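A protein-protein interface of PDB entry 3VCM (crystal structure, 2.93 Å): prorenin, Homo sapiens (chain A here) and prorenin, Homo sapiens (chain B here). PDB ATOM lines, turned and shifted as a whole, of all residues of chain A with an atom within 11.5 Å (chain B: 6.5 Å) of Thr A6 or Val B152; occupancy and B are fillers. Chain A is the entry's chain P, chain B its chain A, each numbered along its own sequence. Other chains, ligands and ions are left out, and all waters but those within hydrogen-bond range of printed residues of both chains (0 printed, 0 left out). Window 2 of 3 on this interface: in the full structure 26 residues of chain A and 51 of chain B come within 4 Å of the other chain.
Of the 12 printed residues of chain B, 4 touch a printed residue of chain A.
Hydrophobic or aromatic side chains of chain B within 4 Å of the printed part of chain A: Ile B102, Val B152 and Leu B173.
Hydrophobic or aromatic side chains of chain A within 4 Å of the printed part of chain B: Phe A8.
Among the printed residues, 5 pairs touch across the chains.
Among the printed residues, no Asp or Glu carboxylate lies within 4 Å of a Lys or Arg side-chain nitrogen of the other chain.
The backbone NH (N) of Thr A6 is in hydrogen-bond range of the backbone carbonyl oxygen (O) of Val B152.
The backbone carbonyl oxygen (O) of Lys A9 lies within hydrogen-bond range of the backbone NH (N) of Leu B173 (2.7 Å).
No residue of chain A comes within 4 Å of Gly B151.
No residue of chain A comes within 4 Å of Lys B154.
Of the printed residues of chain A, Leu B173 touches Lys A9 (2.7 Å).
Printed residues of chain B within 4 Å of Phe A8: Gly B174 (3.98 Å).
Ile B148 touches none of the printed residues of chain A.
Ile B147 touches none of the printed residues of chain A.
The nearest residue of chain B that does not touch Thr A6 is Lys B154 (4.1 Å).
The nearest residue of chain A that does not touch Val B152 is Thr A7 (5.6 Å).
The nearest printed residue of chain A that does not touch Leu B173 is Phe A8 (4.3 Å).
Among the printed residues, merely in contact across the chains: Phe A8 with Gly B174 (3.98 Å), Lys A9 with Ile B102 (3.8 Å) and Lys A9 with Val B152 (3.6 Å).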
ATOM      1  N   THR A   6     -17.813 -19.575  10.607  1.00  0.00           N
ATOM      2  CA  THR A   6     -19.145 -18.963  10.623  1.00  0.00           C
ATOM      3  C   THR A   6     -19.162 -17.550   9.983  1.00  0.00           C
ATOM      4  O   THR A   6     -20.092 -17.220   9.239  1.00  0.00           O
ATOM      5  CB  THR A   6     -19.824 -19.155  12.017  1.00  0.00           C
ATOM      6  OG1 THR A   6     -21.233 -19.357  11.869  1.00  0.00           O
ATOM      7  CG2 THR A   6     -19.499 -18.050  13.029  1.00  0.00           C
ATOM      8  N   THR A   7     -18.101 -16.752  10.256  1.00  0.00           N
ATOM      9  CA  THR A   7     -17.870 -15.390   9.754  1.00  0.00           C
ATOM     10  C   THR A   7     -16.675 -15.363   8.779  1.00  0.00           C
ATOM     11  O   THR A   7     -16.470 -14.365   8.076  1.00  0.00           O
ATOM     12  CB  THR A   7     -17.673 -14.400  10.939  1.00  0.00           C
ATOM     13  OG1 THR A   7     -17.552 -13.072  10.422  1.00  0.00           O
ATOM     14  CG2 THR A   7     -16.449 -14.738  11.819  1.00  0.00           C
ATOM     15  N   PHE A   8     -15.913 -16.494   8.758  1.00  0.00           N
ATOM     16  CA  PHE A   8     -14.660 -16.834   8.055  1.00  0.00           C
ATOM     17  C   PHE A   8     -13.524 -16.837   9.073  1.00  0.00           C
ATOM     18  O   PHE A   8     -13.037 -15.770   9.470  1.00  0.00           O
ATOM     19  CB  PHE A   8     -14.333 -15.920   6.844  1.00  0.00           C
ATOM     20  CG  PHE A   8     -14.586 -16.466   5.451  1.00  0.00           C
ATOM     21  CD1 PHE A   8     -15.272 -17.663   5.263  1.00  0.00           C
ATOM     22  CD2 PHE A   8     -14.156 -15.771   4.327  1.00  0.00           C
ATOM     23  CE1 PHE A   8     -15.513 -18.160   3.973  1.00  0.00           C
ATOM     24  CE2 PHE A   8     -14.392 -16.271   3.036  1.00  0.00           C
ATOM     25  CZ  PHE A   8     -15.069 -17.464   2.868  1.00  0.00           C
ATOM     26  N   LYS A   9     -13.152 -18.038   9.546  1.00  0.00           N
ATOM     27  CA  LYS A   9     -12.059 -18.228  10.499  1.00  0.00           C
ATOM     28  C   LYS A   9     -10.760 -18.332   9.713  1.00  0.00           C
ATOM     29  O   LYS A   9     -10.719 -19.042   8.711  1.00  0.00           O
ATOM     30  CB  LYS A   9     -12.298 -19.482  11.357  1.00  0.00           C
ATOM     31  CG  LYS A   9     -13.228 -19.262  12.552  1.00  0.00           C
ATOM     32  CD  LYS A   9     -14.715 -19.394  12.210  1.00  0.00           C
ATOM     33  CE  LYS A   9     -15.618 -19.034  13.372  1.00  0.00           C
ATOM     34  NZ  LYS A   9     -15.614 -17.573  13.679  1.00  0.00           N
ATOM     35  N   ARG A  10      -9.724 -17.593  10.131  1.00  0.00           N
ATOM     36  CA  ARG A  10      -8.438 -17.560   9.431  1.00  0.00           C
ATOM     37  C   ARG A  10      -7.255 -17.974  10.303  1.00  0.00           C
ATOM     38  O   ARG A  10      -7.164 -17.555  11.458  1.00  0.00           O
ATOM     39  CB  ARG A  10      -8.172 -16.151   8.858  1.00  0.00           C
ATOM     40  CG  ARG A  10      -9.155 -15.707   7.783  1.00  0.00           C
ATOM     41  CD  ARG A  10      -9.034 -14.223   7.484  1.00  0.00           C
ATOM     42  NE  ARG A  10     -10.298 -13.658   7.007  1.00  0.00           N
ATOM     43  CZ  ARG A  10     -10.685 -13.627   5.735  1.00  0.00           C
ATOM     44  NH1 ARG A  10      -9.912 -14.130   4.782  1.00  0.00           N
ATOM     45  NH2 ARG A  10     -11.855 -13.094   5.408  1.00  0.00           N
ATOM     46  N   ILE B 102     -11.161 -21.504  16.628  1.00  0.00           N
ATOM     47  CA  ILE B 102     -11.841 -22.797  16.763  1.00  0.00           C
ATOM     48  C   ILE B 102     -11.139 -23.650  17.812  1.00  0.00           C
ATOM     49  O   ILE B 102      -9.946 -23.915  17.681  1.00  0.00           O
ATOM     50  CB  ILE B 102     -11.998 -23.538  15.401  1.00  0.00           C
ATOM     51  CG1 ILE B 102     -12.711 -22.642  14.354  1.00  0.00           C
ATOM     52  CG2 ILE B 102     -12.735 -24.878  15.579  1.00  0.00           C
ATOM     53  CD1 ILE B 102     -12.398 -22.968  12.901  1.00  0.00           C
ATOM     54  N   THR B 103     -11.893 -24.090  18.834  1.00  0.00           N
ATOM     55  CA  THR B 103     -11.417 -24.933  19.937  1.00  0.00           C
ATOM     56  C   THR B 103     -12.000 -26.342  19.763  1.00  0.00           C
ATOM     57  O   THR B 103     -13.207 -26.476  19.549  1.00  0.00           O
ATOM     58  CB  THR B 103     -11.767 -24.263  21.285  1.00  0.00           C
ATOM     59  OG1 THR B 103     -11.160 -22.972  21.329  1.00  0.00           O
ATOM     60  CG2 THR B 103     -11.296 -25.062  22.484  1.00  0.00           C
ATOM     61  N   ILE B 147     -12.844 -30.334  13.735  1.00  0.00           N
ATOM     62  CA  ILE B 147     -13.354 -28.976  13.493  1.00  0.00           C
ATOM     63  C   ILE B 147     -14.734 -29.071  12.816  1.00  0.00           C
ATOM     64  O   ILE B 147     -15.648 -28.354  13.220  1.00  0.00           O
ATOM     65  CB  ILE B 147     -12.342 -28.116  12.677  1.00  0.00           C
ATOM     66  CG1 ILE B 147     -11.042 -27.856  13.488  1.00  0.00           C
ATOM     67  CG2 ILE B 147     -12.972 -26.792  12.199  1.00  0.00           C
ATOM     68  CD1 ILE B 147      -9.792 -27.402  12.650  1.00  0.00           C
ATOM     69  N   ILE B 148     -14.883 -29.985  11.822  1.00  0.00           N
ATOM     70  CA  ILE B 148     -16.130 -30.244  11.086  1.00  0.00           C
ATOM     71  C   ILE B 148     -17.290 -30.614  12.031  1.00  0.00           C
ATOM     72  O   ILE B 148     -18.375 -30.037  11.913  1.00  0.00           O
ATOM     73  CB  ILE B 148     -15.916 -31.288   9.942  1.00  0.00           C
ATOM     74  CG1 ILE B 148     -15.242 -30.646   8.702  1.00  0.00           C
ATOM     75  CG2 ILE B 148     -17.223 -32.004   9.544  1.00  0.00           C
ATOM     76  CD1 ILE B 148     -14.646 -31.660   7.712  1.00  0.00           C
ATOM     77  N   SER B 149     -17.044 -31.535  12.985  1.00  0.00           N
ATOM     78  CA  SER B 149     -18.051 -31.990  13.958  1.00  0.00           C
ATOM     79  C   SER B 149     -18.508 -30.925  14.973  1.00  0.00           C
ATOM     80  O   SER B 149     -19.497 -31.142  15.679  1.00  0.00           O
ATOM     81  CB  SER B 149     -17.631 -33.291  14.645  1.00  0.00           C
ATOM     82  OG  SER B 149     -16.266 -33.608  14.439  1.00  0.00           O
ATOM     83  N   GLN B 150     -17.823 -29.772  15.018  1.00  0.00           N
ATOM     84  CA  GLN B 150     -18.202 -28.662  15.895  1.00  0.00           C
ATOM     85  C   GLN B 150     -19.326 -27.822  15.270  1.00  0.00           C
ATOM     86  O   GLN B 150     -19.978 -27.056  15.980  1.00  0.00           O
ATOM     87  CB  GLN B 150     -16.995 -27.755  16.210  1.00  0.00           C
ATOM     88  CG  GLN B 150     -15.785 -28.438  16.839  1.00  0.00           C
ATOM     89  CD  GLN B 150     -16.050 -29.041  18.196  1.00  0.00           C
ATOM     90  OE1 GLN B 150     -15.979 -30.262  18.374  1.00  0.00           O
ATOM     91  NE2 GLN B 150     -16.341 -28.202  19.184  1.00  0.00           N
ATOM     92  N   GLY B 151     -19.520 -27.953  13.957  1.00  0.00           N
ATOM     93  CA  GLY B 151     -20.528 -27.215  13.202  1.00  0.00           C
ATOM     94  C   GLY B 151     -20.335 -25.711  13.260  1.00  0.00           C
ATOM     95  O   GLY B 151     -21.304 -24.952  13.352  1.00  0.00           O
ATOM     96  N   VAL B 152     -19.075 -25.280  13.221  1.00  0.00           N
ATOM     97  CA  VAL B 152     -18.687 -23.878  13.284  1.00  0.00           C
ATOM     98  C   VAL B 152     -18.485 -23.330  11.861  1.00  0.00           C
ATOM     99  O   VAL B 152     -18.809 -22.176  11.602  1.00  0.00           O
ATOM    100  CB  VAL B 152     -17.448 -23.691  14.209  1.00  0.00           C
ATOM    101  CG1 VAL B 152     -16.993 -22.240  14.270  1.00  0.00           C
ATOM    102  CG2 VAL B 152     -17.737 -24.198  15.613  1.00  0.00           C
ATOM    103  N   LEU B 153     -18.001 -24.171  10.937  1.00  0.00           N
ATOM    104  CA  LEU B 153     -17.718 -23.775   9.552  1.00  0.00           C
ATOM    105  C   LEU B 153     -18.954 -23.592   8.669  1.00  0.00           C
ATOM    106  O   LEU B 153     -19.954 -24.294   8.840  1.00  0.00           O
ATOM    107  CB  LEU B 153     -16.761 -24.778   8.888  1.00  0.00           C
ATOM    108  CG  LEU B 153     -15.475 -25.135   9.638  1.00  0.00           C
ATOM    109  CD1 LEU B 153     -14.744 -26.213   8.904  1.00  0.00           C
ATOM    110  CD2 LEU B 153     -14.563 -23.926   9.820  1.00  0.00           C
ATOM    111  N   LYS B 154     -18.854 -22.673   7.693  1.00  0.00           N
ATOM    112  CA  LYS B 154     -19.911 -22.400   6.711  1.00  0.00           C
ATOM    113  C   LYS B 154     -19.968 -23.572   5.709  1.00  0.00           C
ATOM    114  O   LYS B 154     -21.049 -24.069   5.390  1.00  0.00           O
ATOM    115  CB  LYS B 154     -19.647 -21.061   5.996  1.00  0.00           C
ATOM    116  CG  LYS B 154     -20.918 -20.351   5.538  1.00  0.00           C
ATOM    117  CD  LYS B 154     -20.744 -18.827   5.479  1.00  0.00           C
ATOM    118  CE  LYS B 154     -20.468 -18.309   4.081  1.00  0.00           C
ATOM    119  NZ  LYS B 154     -20.325 -16.825   4.056  1.00  0.00           N
ATOM    120  N   LEU B 173     -10.620 -21.064   6.906  1.00  0.00           N
ATOM    121  CA  LEU B 173     -11.407 -22.191   7.418  1.00  0.00           C
ATOM    122  C   LEU B 173     -12.908 -21.949   7.223  1.00  0.00           C
ATOM    123  O   LEU B 173     -13.444 -20.953   7.722  1.00  0.00           O
ATOM    124  CB  LEU B 173     -11.106 -22.438   8.908  1.00  0.00           C
ATOM    125  CG  LEU B 173      -9.706 -22.919   9.282  1.00  0.00           C
ATOM    126  CD1 LEU B 173      -9.441 -22.641  10.732  1.00  0.00           C
ATOM    127  CD2 LEU B 173      -9.537 -24.408   9.019  1.00  0.00           C
ATOM    128  N   GLY B 174     -13.567 -22.861   6.506  1.00  0.00           N
ATOM    129  CA  GLY B 174     -15.003 -22.792   6.248  1.00  0.00           C
ATOM    130  C   GLY B 174     -15.415 -22.200   4.914  1.00  0.00           C
ATOM    131  O   GLY B 174     -16.599 -21.922   4.702  1.00  0.00           O
